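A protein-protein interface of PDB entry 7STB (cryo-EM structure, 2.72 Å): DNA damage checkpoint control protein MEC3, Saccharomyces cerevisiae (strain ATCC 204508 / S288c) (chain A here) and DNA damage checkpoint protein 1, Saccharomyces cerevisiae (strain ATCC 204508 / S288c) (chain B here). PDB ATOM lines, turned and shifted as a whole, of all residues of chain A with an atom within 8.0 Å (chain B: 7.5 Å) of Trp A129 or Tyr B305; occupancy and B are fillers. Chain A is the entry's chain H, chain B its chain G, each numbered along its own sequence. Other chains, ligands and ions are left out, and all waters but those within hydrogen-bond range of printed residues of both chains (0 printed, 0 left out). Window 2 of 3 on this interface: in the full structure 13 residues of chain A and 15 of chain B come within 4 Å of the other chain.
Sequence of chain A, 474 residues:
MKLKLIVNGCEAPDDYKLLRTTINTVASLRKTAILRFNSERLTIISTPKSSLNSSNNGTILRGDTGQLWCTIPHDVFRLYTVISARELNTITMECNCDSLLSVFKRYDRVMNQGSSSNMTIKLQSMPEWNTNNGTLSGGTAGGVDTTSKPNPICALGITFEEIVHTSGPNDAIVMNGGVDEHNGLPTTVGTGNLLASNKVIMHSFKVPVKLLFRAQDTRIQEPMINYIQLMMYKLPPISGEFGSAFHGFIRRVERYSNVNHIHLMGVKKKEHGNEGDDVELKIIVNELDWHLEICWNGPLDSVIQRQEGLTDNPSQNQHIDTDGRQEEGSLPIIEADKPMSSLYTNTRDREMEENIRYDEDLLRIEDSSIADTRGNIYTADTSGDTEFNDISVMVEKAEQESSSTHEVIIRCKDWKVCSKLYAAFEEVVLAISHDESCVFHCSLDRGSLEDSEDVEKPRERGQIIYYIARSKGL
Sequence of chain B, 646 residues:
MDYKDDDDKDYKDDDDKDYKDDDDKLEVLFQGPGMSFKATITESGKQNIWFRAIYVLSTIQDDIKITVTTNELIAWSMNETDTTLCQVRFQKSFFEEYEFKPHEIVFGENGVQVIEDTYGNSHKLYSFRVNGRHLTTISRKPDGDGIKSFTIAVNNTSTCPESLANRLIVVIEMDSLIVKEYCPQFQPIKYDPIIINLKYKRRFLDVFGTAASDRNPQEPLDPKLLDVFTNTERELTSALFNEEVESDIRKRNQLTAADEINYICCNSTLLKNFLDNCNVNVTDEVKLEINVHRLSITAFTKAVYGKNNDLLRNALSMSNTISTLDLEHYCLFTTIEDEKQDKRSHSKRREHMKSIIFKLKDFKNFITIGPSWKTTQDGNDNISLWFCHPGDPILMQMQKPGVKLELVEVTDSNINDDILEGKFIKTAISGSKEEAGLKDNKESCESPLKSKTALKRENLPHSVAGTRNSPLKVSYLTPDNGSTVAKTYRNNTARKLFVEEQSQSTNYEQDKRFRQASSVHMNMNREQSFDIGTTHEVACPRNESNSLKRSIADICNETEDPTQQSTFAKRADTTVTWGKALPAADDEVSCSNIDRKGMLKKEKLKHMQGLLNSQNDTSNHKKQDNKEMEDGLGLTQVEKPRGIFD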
ATOM      1  N   GLN A 124      -0.237 -18.553   1.382  1.00  0.00           N
ATOM      2  CA  GLN A 124       1.132 -18.145   1.654  1.00  0.00           C
ATOM      3  C   GLN A 124       1.978 -18.300   0.398  1.00  0.00           C
ATOM      4  O   GLN A 124       1.699 -19.138  -0.461  1.00  0.00           O
ATOM      5  CB  GLN A 124       1.744 -18.971   2.793  1.00  0.00           C
ATOM      6  CG  GLN A 124       1.043 -18.794   4.131  1.00  0.00           C
ATOM      7  CD  GLN A 124       1.176 -20.007   5.033  1.00  0.00           C
ATOM      8  OE1 GLN A 124       1.633 -21.067   4.608  1.00  0.00           O
ATOM      9  NE2 GLN A 124       0.776 -19.852   6.290  1.00  0.00           N
ATOM     10  N   SER A 125       3.016 -17.476   0.302  1.00  0.00           N
ATOM     11  CA  SER A 125       3.963 -17.554  -0.797  1.00  0.00           C
ATOM     12  C   SER A 125       5.101 -18.489  -0.417  1.00  0.00           C
ATOM     13  O   SER A 125       5.544 -18.524   0.735  1.00  0.00           O
ATOM     14  CB  SER A 125       4.509 -16.169  -1.148  1.00  0.00           C
ATOM     15  OG  SER A 125       5.265 -15.631  -0.078  1.00  0.00           O
ATOM     16  N   MET A 126       5.569 -19.258  -1.400  1.00  0.00           N
ATOM     17  CA  MET A 126       6.570 -20.300  -1.184  1.00  0.00           C
ATOM     18  C   MET A 126       7.815 -19.979  -2.000  1.00  0.00           C
ATOM     19  O   MET A 126       7.905 -20.343  -3.183  1.00  0.00           O
ATOM     20  CB  MET A 126       6.007 -21.671  -1.555  1.00  0.00           C
ATOM     21  CG  MET A 126       4.865 -22.125  -0.657  1.00  0.00           C
ATOM     22  SD  MET A 126       5.350 -22.283   1.072  1.00  0.00           S
ATOM     23  CE  MET A 126       6.442 -23.700   1.001  1.00  0.00           C
ATOM     24  N   PRO A 127       8.803 -19.298  -1.410  1.00  0.00           N
ATOM     25  CA  PRO A 127      10.076 -19.094  -2.112  1.00  0.00           C
ATOM     26  C   PRO A 127      11.011 -20.288  -2.029  1.00  0.00           C
ATOM     27  O   PRO A 127      11.989 -20.341  -2.788  1.00  0.00           O
ATOM     28  CB  PRO A 127      10.681 -17.870  -1.403  1.00  0.00           C
ATOM     29  CG  PRO A 127       9.880 -17.671  -0.134  1.00  0.00           C
ATOM     30  CD  PRO A 127       8.825 -18.730  -0.053  1.00  0.00           C
ATOM     31  N   GLU A 128      10.744 -21.241  -1.132  1.00  0.00           N
ATOM     32  CA  GLU A 128      11.555 -22.450  -1.072  1.00  0.00           C
ATOM     33  C   GLU A 128      11.329 -23.336  -2.290  1.00  0.00           C
ATOM     34  O   GLU A 128      12.264 -23.998  -2.756  1.00  0.00           O
ATOM     35  CB  GLU A 128      11.247 -23.222   0.210  1.00  0.00           C
ATOM     36  CG  GLU A 128      12.171 -24.402   0.462  1.00  0.00           C
ATOM     37  CD  GLU A 128      12.091 -24.914   1.888  1.00  0.00           C
ATOM     38  OE1 GLU A 128      11.844 -24.099   2.802  1.00  0.00           O
ATOM     39  OE2 GLU A 128      12.272 -26.132   2.095  1.00  0.00           O
ATOM     40  N   TRP A 129      10.108 -23.364  -2.814  1.00  0.00           N
ATOM     41  CA  TRP A 129       9.802 -24.152  -4.002  1.00  0.00           C
ATOM     42  C   TRP A 129      10.309 -23.443  -5.252  1.00  0.00           C
ATOM     43  O   TRP A 129      10.522 -22.231  -5.247  1.00  0.00           O
ATOM     44  CB  TRP A 129       8.296 -24.403  -4.114  1.00  0.00           C
ATOM     45  CG  TRP A 129       7.711 -25.143  -2.946  1.00  0.00           C
ATOM     46  CD1 TRP A 129       8.392 -25.737  -1.923  1.00  0.00           C
ATOM     47  CD2 TRP A 129       6.321 -25.374  -2.686  1.00  0.00           C
ATOM     48  NE1 TRP A 129       7.514 -26.319  -1.042  1.00  0.00           N
ATOM     49  CE2 TRP A 129       6.235 -26.111  -1.488  1.00  0.00           C
ATOM     50  CE3 TRP A 129       5.138 -25.028  -3.350  1.00  0.00           C
ATOM     51  CZ2 TRP A 129       5.018 -26.507  -0.940  1.00  0.00           C
ATOM     52  CZ3 TRP A 129       3.932 -25.422  -2.804  1.00  0.00           C
ATOM     53  CH2 TRP A 129       3.880 -26.155  -1.611  1.00  0.00           C
ATOM     54  N   ILE A 153       3.117 -19.751  -8.025  1.00  0.00           N
ATOM     55  CA  ILE A 153       2.734 -20.954  -7.295  1.00  0.00           C
ATOM     56  C   ILE A 153       2.816 -20.641  -5.808  1.00  0.00           C
ATOM     57  O   ILE A 153       3.862 -20.200  -5.315  1.00  0.00           O
ATOM     58  CB  ILE A 153       3.627 -22.149  -7.664  1.00  0.00           C
ATOM     59  CG1 ILE A 153       3.332 -22.583  -9.105  1.00  0.00           C
ATOM     60  CG2 ILE A 153       3.413 -23.302  -6.680  1.00  0.00           C
ATOM     61  CD1 ILE A 153       4.057 -23.833  -9.545  1.00  0.00           C
ATOM     62  N   CYS A 154       1.713 -20.872  -5.096  1.00  0.00           N
ATOM     63  CA  CYS A 154       1.636 -20.585  -3.670  1.00  0.00           C
ATOM     64  C   CYS A 154       1.194 -21.827  -2.909  1.00  0.00           C
ATOM     65  O   CYS A 154       1.081 -22.911  -3.490  1.00  0.00           O
ATOM     66  CB  CYS A 154       0.674 -19.422  -3.418  1.00  0.00           C
ATOM     67  SG  CYS A 154       1.228 -17.846  -4.105  1.00  0.00           S
ATOM     68  N   ALA A 155       0.933 -21.684  -1.612  1.00  0.00           N
ATOM     69  CA  ALA A 155       0.526 -22.800  -0.776  1.00  0.00           C
ATOM     70  C   ALA A 155      -0.651 -22.398   0.100  1.00  0.00           C
ATOM     71  O   ALA A 155      -0.841 -21.222   0.421  1.00  0.00           O
ATOM     72  CB  ALA A 155       1.682 -23.291   0.106  1.00  0.00           C
ATOM     73  N   LEU A 156      -1.448 -23.396   0.464  1.00  0.00           N
ATOM     74  CA  LEU A 156      -2.517 -23.247   1.439  1.00  0.00           C
ATOM     75  C   LEU A 156      -2.045 -23.867   2.747  1.00  0.00           C
ATOM     76  O   LEU A 156      -1.727 -25.062   2.791  1.00  0.00           O
ATOM     77  CB  LEU A 156      -3.802 -23.917   0.953  1.00  0.00           C
ATOM     78  CG  LEU A 156      -4.653 -23.114  -0.034  1.00  0.00           C
ATOM     79  CD1 LEU A 156      -5.796 -23.963  -0.565  1.00  0.00           C
ATOM     80  CD2 LEU A 156      -5.184 -21.847   0.617  1.00  0.00           C
ATOM     81  N   PHE A 205      -0.677 -28.491   7.049  1.00  0.00           N
ATOM     82  CA  PHE A 205      -0.609 -28.997   5.684  1.00  0.00           C
ATOM     83  C   PHE A 205      -0.355 -27.829   4.746  1.00  0.00           C
ATOM     84  O   PHE A 205      -1.147 -26.884   4.704  1.00  0.00           O
ATOM     85  CB  PHE A 205      -1.902 -29.721   5.293  1.00  0.00           C
ATOM     86  CG  PHE A 205      -2.402 -30.676   6.337  1.00  0.00           C
ATOM     87  CD1 PHE A 205      -3.140 -30.220   7.415  1.00  0.00           C
ATOM     88  CD2 PHE A 205      -2.139 -32.031   6.238  1.00  0.00           C
ATOM     89  CE1 PHE A 205      -3.598 -31.093   8.377  1.00  0.00           C
ATOM     90  CE2 PHE A 205      -2.600 -32.909   7.197  1.00  0.00           C
ATOM     91  CZ  PHE A 205      -3.330 -32.439   8.267  1.00  0.00           C
ATOM     92  N   LYS A 206       0.745 -27.898   3.997  1.00  0.00           N
ATOM     93  CA  LYS A 206       1.073 -26.905   2.975  1.00  0.00           C
ATOM     94  C   LYS A 206       0.683 -27.506   1.630  1.00  0.00           C
ATOM     95  O   LYS A 206       1.466 -28.210   0.991  1.00  0.00           O
ATOM     96  CB  LYS A 206       2.551 -26.534   3.020  1.00  0.00           C
ATOM     97  CG  LYS A 206       3.022 -25.989   4.357  1.00  0.00           C
ATOM     98  CD  LYS A 206       2.516 -24.576   4.596  1.00  0.00           C
ATOM     99  CE  LYS A 206       3.083 -23.997   5.882  1.00  0.00           C
ATOM    100  NZ  LYS A 206       2.575 -22.623   6.152  1.00  0.00           N
ATOM    101  N   VAL A 207      -0.541 -27.225   1.199  1.00  0.00           N
ATOM    102  CA  VAL A 207      -1.087 -27.787  -0.032  1.00  0.00           C
ATOM    103  C   VAL A 207      -0.665 -26.886  -1.191  1.00  0.00           C
ATOM    104  O   VAL A 207      -1.003 -25.695  -1.181  1.00  0.00           O
ATOM    105  CB  VAL A 207      -2.614 -27.908   0.037  1.00  0.00           C
ATOM    106  CG1 VAL A 207      -3.164 -28.457  -1.272  1.00  0.00           C
ATOM    107  CG2 VAL A 207      -3.023 -28.791   1.205  1.00  0.00           C
ATOM    108  N   PRO A 208       0.053 -27.397  -2.192  1.00  0.00           N
ATOM    109  CA  PRO A 208       0.422 -26.545  -3.327  1.00  0.00           C
ATOM    110  C   PRO A 208      -0.812 -26.070  -4.080  1.00  0.00           C
ATOM    111  O   PRO A 208      -1.835 -26.756  -4.131  1.00  0.00           O
ATOM    112  CB  PRO A 208       1.294 -27.459  -4.194  1.00  0.00           C
ATOM    113  CG  PRO A 208       0.861 -28.834  -3.843  1.00  0.00           C
ATOM    114  CD  PRO A 208       0.495 -28.790  -2.389  1.00  0.00           C
ATOM    115  N   VAL A 209      -0.707 -24.881  -4.670  1.00  0.00           N
ATOM    116  CA  VAL A 209      -1.816 -24.288  -5.410  1.00  0.00           C
ATOM    117  C   VAL A 209      -1.231 -23.299  -6.406  1.00  0.00           C
ATOM    118  O   VAL A 209      -0.122 -22.797  -6.225  1.00  0.00           O
ATOM    119  CB  VAL A 209      -2.825 -23.609  -4.449  1.00  0.00           C
ATOM    120  CG1 VAL A 209      -2.250 -22.315  -3.889  1.00  0.00           C
ATOM    121  CG2 VAL A 209      -4.144 -23.362  -5.148  1.00  0.00           C
ATOM    122  N   LYS A 210      -1.976 -23.029  -7.474  1.00  0.00           N
ATOM    123  CA  LYS A 210      -1.539 -22.124  -8.530  1.00  0.00           C
ATOM    124  C   LYS A 210      -2.490 -20.938  -8.611  1.00  0.00           C
ATOM    125  O   LYS A 210      -3.699 -21.119  -8.772  1.00  0.00           O
ATOM    126  CB  LYS A 210      -1.484 -22.849  -9.877  1.00  0.00           C
ATOM    127  CG  LYS A 210      -0.675 -22.128 -10.941  1.00  0.00           C
ATOM    128  CD  LYS A 210      -1.240 -22.367 -12.333  1.00  0.00           C
ATOM    129  CE  LYS A 210      -1.214 -23.843 -12.709  1.00  0.00           C
ATOM    130  NZ  LYS A 210      -1.837 -24.088 -14.039  1.00  0.00           N
ATOM    131  N   THR B 301       7.979 -33.719   0.025  1.00  0.00           N
ATOM    132  CA  THR B 301       8.549 -33.988  -1.284  1.00  0.00           C
ATOM    133  C   THR B 301       9.229 -32.722  -1.785  1.00  0.00           C
ATOM    134  O   THR B 301       8.820 -31.608  -1.447  1.00  0.00           O
ATOM    135  CB  THR B 301       7.469 -34.434  -2.284  1.00  0.00           C
ATOM    136  OG1 THR B 301       6.840 -35.631  -1.811  1.00  0.00           O
ATOM    137  CG2 THR B 301       8.068 -34.688  -3.660  1.00  0.00           C
ATOM    138  N   LYS B 302      10.274 -32.897  -2.588  1.00  0.00           N
ATOM    139  CA  LYS B 302      11.002 -31.773  -3.161  1.00  0.00           C
ATOM    140  C   LYS B 302      10.492 -31.497  -4.570  1.00  0.00           C
ATOM    141  O   LYS B 302      10.349 -32.420  -5.377  1.00  0.00           O
ATOM    142  CB  LYS B 302      12.505 -32.054  -3.195  1.00  0.00           C
ATOM    143  CG  LYS B 302      13.156 -32.167  -1.829  1.00  0.00           C
ATOM    144  CD  LYS B 302      14.649 -32.430  -1.959  1.00  0.00           C
ATOM    145  CE  LYS B 302      15.342 -32.461  -0.606  1.00  0.00           C
ATOM    146  NZ  LYS B 302      14.909 -33.622   0.217  1.00  0.00           N
ATOM    147  N   ALA B 303      10.215 -30.228  -4.857  1.00  0.00           N
ATOM    148  CA  ALA B 303       9.767 -29.846  -6.189  1.00  0.00           C
ATOM    149  C   ALA B 303      10.908 -29.970  -7.190  1.00  0.00           C
ATOM    150  O   ALA B 303      12.066 -29.680  -6.878  1.00  0.00           O
ATOM    151  CB  ALA B 303       9.232 -28.415  -6.179  1.00  0.00           C
ATOM    152  N   VAL B 304      10.575 -30.408  -8.401  1.00  0.00           N
ATOM    153  CA  VAL B 304      11.530 -30.541  -9.493  1.00  0.00           C
ATOM    154  C   VAL B 304      11.023 -29.713 -10.665  1.00  0.00           C
ATOM    155  O   VAL B 304       9.855 -29.833 -11.054  1.00  0.00           O
ATOM    156  CB  VAL B 304      11.726 -32.012  -9.905  1.00  0.00           C
ATOM    157  CG1 VAL B 304      12.861 -32.138 -10.908  1.00  0.00           C
ATOM    158  CG2 VAL B 304      11.992 -32.878  -8.682  1.00  0.00           C
ATOM    159  N   TYR B 305      11.897 -28.881 -11.222  1.00  0.00           N
ATOM    160  CA  TYR B 305      11.549 -27.978 -12.309  1.00  0.00           C
ATOM    161  C   TYR B 305      12.286 -28.383 -13.578  1.00  0.00           C
ATOM    162  O   TYR B 305      13.470 -28.729 -13.538  1.00  0.00           O
ATOM    163  CB  TYR B 305      11.886 -26.531 -11.942  1.00  0.00           C
ATOM    164  CG  TYR B 305      10.944 -25.938 -10.922  1.00  0.00           C
ATOM    165  CD1 TYR B 305       9.657 -25.557 -11.277  1.00  0.00           C
ATOM    166  CD2 TYR B 305      11.335 -25.768  -9.602  1.00  0.00           C
ATOM    167  CE1 TYR B 305       8.790 -25.017 -10.348  1.00  0.00           C
ATOM    168  CE2 TYR B 305      10.475 -25.229  -8.666  1.00  0.00           C
ATOM    169  CZ  TYR B 305       9.203 -24.856  -9.044  1.00  0.00           C
ATOM    170  OH  TYR B 305       8.343 -24.319  -8.116  1.00  0.00           O
ATOM    171  N   GLY B 306      11.578 -28.330 -14.704  1.00  0.00           N
ATOM    172  CA  GLY B 306      12.121 -28.787 -15.967  1.00  0.00           C
ATOM    173  C   GLY B 306      12.821 -27.708 -16.767  1.00  0.00           C
ATOM    174  O   GLY B 306      13.504 -26.847 -16.206  1.00  0.00           O
ATOM    175  N   LYS B 307      12.658 -27.751 -18.090  1.00  0.00           N
ATOM    176  CA  LYS B 307      13.362 -26.841 -18.984  1.00  0.00           C
ATOM    177  C   LYS B 307      12.991 -25.389 -18.709  1.00  0.00           C
ATOM    178  O   LYS B 307      13.833 -24.602 -18.264  1.00  0.00           O
ATOM    179  CB  LYS B 307      13.052 -27.200 -20.441  1.00  0.00           C
ATOM    180  CG  LYS B 307      13.724 -26.309 -21.479  1.00  0.00           C
ATOM    181  CD  LYS B 307      15.228 -26.515 -21.512  1.00  0.00           C
ATOM    182  CE  LYS B 307      15.877 -25.662 -22.591  1.00  0.00           C
ATOM    183  NZ  LYS B 307      17.342 -25.900 -22.693  1.00  0.00           N
ATOM    184  N   ASN B 308      11.739 -25.025 -18.968  1.00  0.00           N
ATOM    185  CA  ASN B 308      11.279 -23.646 -18.800  1.00  0.00           C
ATOM    186  C   ASN B 308      10.608 -23.464 -17.440  1.00  0.00           C
ATOM    187  O   ASN B 308       9.460 -23.031 -17.331  1.00  0.00           O
ATOM    188  CB  ASN B 308      10.335 -23.267 -19.937  1.00  0.00           C
ATOM    189  CG  ASN B 308      11.041 -23.181 -21.276  1.00  0.00           C
ATOM    190  OD1 ASN B 308      12.216 -22.824 -21.349  1.00  0.00           O
ATOM    191  ND2 ASN B 308      10.324 -23.511 -22.345  1.00  0.00           N
ATOM    192  N   ASN B 309      11.355 -23.796 -16.387  1.00  0.00           N
ATOM    193  CA  ASN B 309      10.869 -23.658 -15.016  1.00  0.00           C
ATOM    194  C   ASN B 309       9.494 -24.301 -14.860  1.00  0.00           C
ATOM    195  O   ASN B 309       8.593 -23.752 -14.221  1.00  0.00           O
ATOM    196  CB  ASN B 309      10.834 -22.188 -14.596  1.00  0.00           C
ATOM    197  CG  ASN B 309      10.822 -22.010 -13.091  1.00  0.00           C
ATOM    198  OD1 ASN B 309      10.890 -22.982 -12.338  1.00  0.00           O
ATOM    199  ND2 ASN B 309      10.736 -20.763 -12.643  1.00  0.00           N
ATOM    200  N   ASP B 310       9.331 -25.480 -15.452  1.00  0.00           N
ATOM    201  CA  ASP B 310       8.062 -26.197 -15.449  1.00  0.00           C
ATOM    202  C   ASP B 310       8.124 -27.331 -14.435  1.00  0.00           C
ATOM    203  O   ASP B 310       9.076 -28.117 -14.433  1.00  0.00           O
ATOM    204  CB  ASP B 310       7.747 -26.744 -16.842  1.00  0.00           C
ATOM    205  CG  ASP B 310       6.370 -27.375 -16.924  1.00  0.00           C
ATOM    206  OD1 ASP B 310       5.591 -27.236 -15.958  1.00  0.00           O
ATOM    207  OD2 ASP B 310       6.070 -28.009 -17.956  1.00  0.00           O
ATOM    208  N   LEU B 311       7.108 -27.413 -13.581  1.00  0.00           N
ATOM    209  CA  LEU B 311       7.086 -28.428 -12.536  1.00  0.00           C
ATOM    210  C   LEU B 311       7.092 -29.823 -13.141  1.00  0.00           C
ATOM    211  O   LEU B 311       6.138 -30.222 -13.818  1.00  0.00           O
ATOM    212  CB  LEU B 311       5.855 -28.245 -11.650  1.00  0.00           C
ATOM    213  CG  LEU B 311       6.022 -27.351 -10.422  1.00  0.00           C
ATOM    214  CD1 LEU B 311       4.663 -27.007  -9.839  1.00  0.00           C
ATOM    215  CD2 LEU B 311       6.899 -28.021  -9.377  1.00  0.00           C
ATOM    216  N   LEU B 312       8.170 -30.565 -12.897  1.00  0.00           N
ATOM    217  CA  LEU B 312       8.222 -31.974 -13.261  1.00  0.00           C
ATOM    218  C   LEU B 312       7.648 -32.877 -12.181  1.00  0.00           C
ATOM    219  O   LEU B 312       7.284 -34.021 -12.476  1.00  0.00           O
ATOM    220  CB  LEU B 312       9.667 -32.396 -13.549  1.00  0.00           C
ATOM    221  CG  LEU B 312      10.380 -31.679 -14.697  1.00  0.00           C
ATOM    222  CD1 LEU B 312      11.799 -32.206 -14.840  1.00  0.00           C
ATOM    223  CD2 LEU B 312       9.616 -31.837 -16.002  1.00  0.00           C
ATOM    224  N   ARG B 313       7.558 -32.394 -10.943  1.00  0.00           N
ATOM    225  CA  ARG B 313       7.017 -33.189  -9.845  1.00  0.00           C
ATOM    226  C   ARG B 313       6.595 -32.233  -8.743  1.00  0.00           C
ATOM    227  O   ARG B 313       7.437 -31.519  -8.190  1.00  0.00           O
ATOM    228  CB  ARG B 313       8.056 -34.190  -9.339  1.00  0.00           C
ATOM    229  CG  ARG B 313       7.556 -35.131  -8.260  1.00  0.00           C
ATOM    230  CD  ARG B 313       8.632 -36.142  -7.898  1.00  0.00           C
ATOM    231  NE  ARG B 313       8.230 -37.025  -6.809  1.00  0.00           N
ATOM    232  CZ  ARG B 313       7.550 -38.153  -6.971  1.00  0.00           C
ATOM    233  NH1 ARG B 313       7.150 -38.555  -8.167  1.00  0.00           N
ATOM    234  NH2 ARG B 313       7.265 -38.896  -5.907  1.00  0.00           N
ATOM    235  N   ASN B 314       5.303 -32.212  -8.430  1.00  0.00           N
ATOM    236  CA  ASN B 314       4.782 -31.251  -7.469  1.00  0.00           C
ATOM    237  C   ASN B 314       5.246 -31.582  -6.055  1.00  0.00           C
ATOM    238  O   ASN B 314       5.525 -32.736  -5.718  1.00  0.00           O
ATOM    239  CB  ASN B 314       3.256 -31.219  -7.520  1.00  0.00           C
ATOM    240  CG  ASN B 314       2.699 -29.815  -7.389  1.00  0.00           C
ATOM    241  OD1 ASN B 314       3.297 -28.957  -6.738  1.00  0.00           O
ATOM    242  ND2 ASN B 314       1.552 -29.571  -8.011  1.00  0.00           N
ATOM    243  N   ALA B 315       5.324 -30.547  -5.223  1.00  0.00           N
ATOM    244  CA  ALA B 315       5.776 -30.670  -3.844  1.00  0.00           C
ATOM    245  C   ALA B 315       4.591 -30.547  -2.896  1.00  0.00           C
ATOM    246  O   ALA B 315       3.795 -29.609  -3.008  1.00  0.00           O
ATOM    247  CB  ALA B 315       6.820 -29.603  -3.518  1.00  0.00           C
ATOM    248  N   LEU B 316       4.482 -31.492  -1.967  1.00  0.00           N
ATOM    249  CA  LEU B 316       3.445 -31.483  -0.947  1.00  0.00           C
ATOM    250  C   LEU B 316       4.082 -31.759   0.406  1.00  0.00           C
ATOM    251  O   LEU B 316       5.075 -32.484   0.503  1.00  0.00           O
ATOM    252  CB  LEU B 316       2.351 -32.524  -1.246  1.00  0.00           C
ATOM    253  CG  LEU B 316       1.306 -32.784  -0.156  1.00  0.00           C
ATOM    254  CD1 LEU B 316       0.303 -31.644  -0.092  1.00  0.00           C
ATOM    255  CD2 LEU B 316       0.599 -34.105  -0.401  1.00  0.00           C
ATOM    256  N   SER B 317       3.504 -31.171   1.450  1.00  0.00           N
ATOM    257  CA  SER B 317       4.007 -31.322   2.806  1.00  0.00           C
ATOM    258  C   SER B 317       2.866 -31.692   3.743  1.00  0.00           C
ATOM    259  O   SER B 317       1.722 -31.270   3.555  1.00  0.00           O
ATOM    260  CB  SER B 317       4.687 -30.037   3.298  1.00  0.00           C
ATOM    261  OG  SER B 317       5.112 -30.169   4.642  1.00  0.00           O
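Of chain B, only Tyr B305 (3.6 Å) and Ala B315 (3.7 Å) come within 4 Å of Trp A129. Ala A155 touches none of the printed residues of chain B. No residue of chain A comes within 4 Å of Gly B306. Of the printed residues of chain A, Asn B314 touches Pro A208 (3.6 Å). Printed residues of chain A within 4 Å of Ala B315: Trp A129 (3.7 Å) and Pro A208 (3.1 Å). Of the printed residues of chain A, Leu B316 touches Lys A206 (3.8 Å) and Pro A208 (3.7 Å). Of the printed residues of chain A, Ser B317 touches Phe A205 (3.9 Å) and Lys A206 (3.5 Å). The nearest residue of chain B that does not touch Trp A129 is Ala B303 (4.6 Å). The nearest residue of chain A that does not touch Tyr B305 is Ile A153 (4.5 Å).
Among the printed residues, pairs that only touch across the chains: Trp A129 with Tyr B305 (3.6 Å), Trp A129 with Ala B315 (3.7 Å), Ile A153 with Leu B311 (3.2 Å), Phe A205 with Ser B317 (3.9 Å), Lys A206 with Leu B316 (3.8 Å), Lys A206 with Ser B317 (3.5 Å), Pro A208 with Asn B314 (3.6 Å), Pro A208 with Ala B315 (3.1 Å) and Pro A208 with Leu B316 (3.7 Å).
Of the 16 printed residues of chain A, 5 touch a printed residue of chain B. Among the printed residues, 9 pairs touch across the chains. Among the printed residues, no Asp or Glu carboxylate lies within 4 Å of a Lys or Arg side-chain nitrogen of the other chain.
The backbone carbonyl oxygen of Leu B316 is in hydrogen-bond range of the backbone NH of Thr B301. NZ of Lys A206 lies close to NE2 of Gln A124 (3.3 Å). The backbone carbonyl oxygen of Leu A156 lies close to the backbone carbonyl oxygen of Phe A205, 2.7 Å away.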
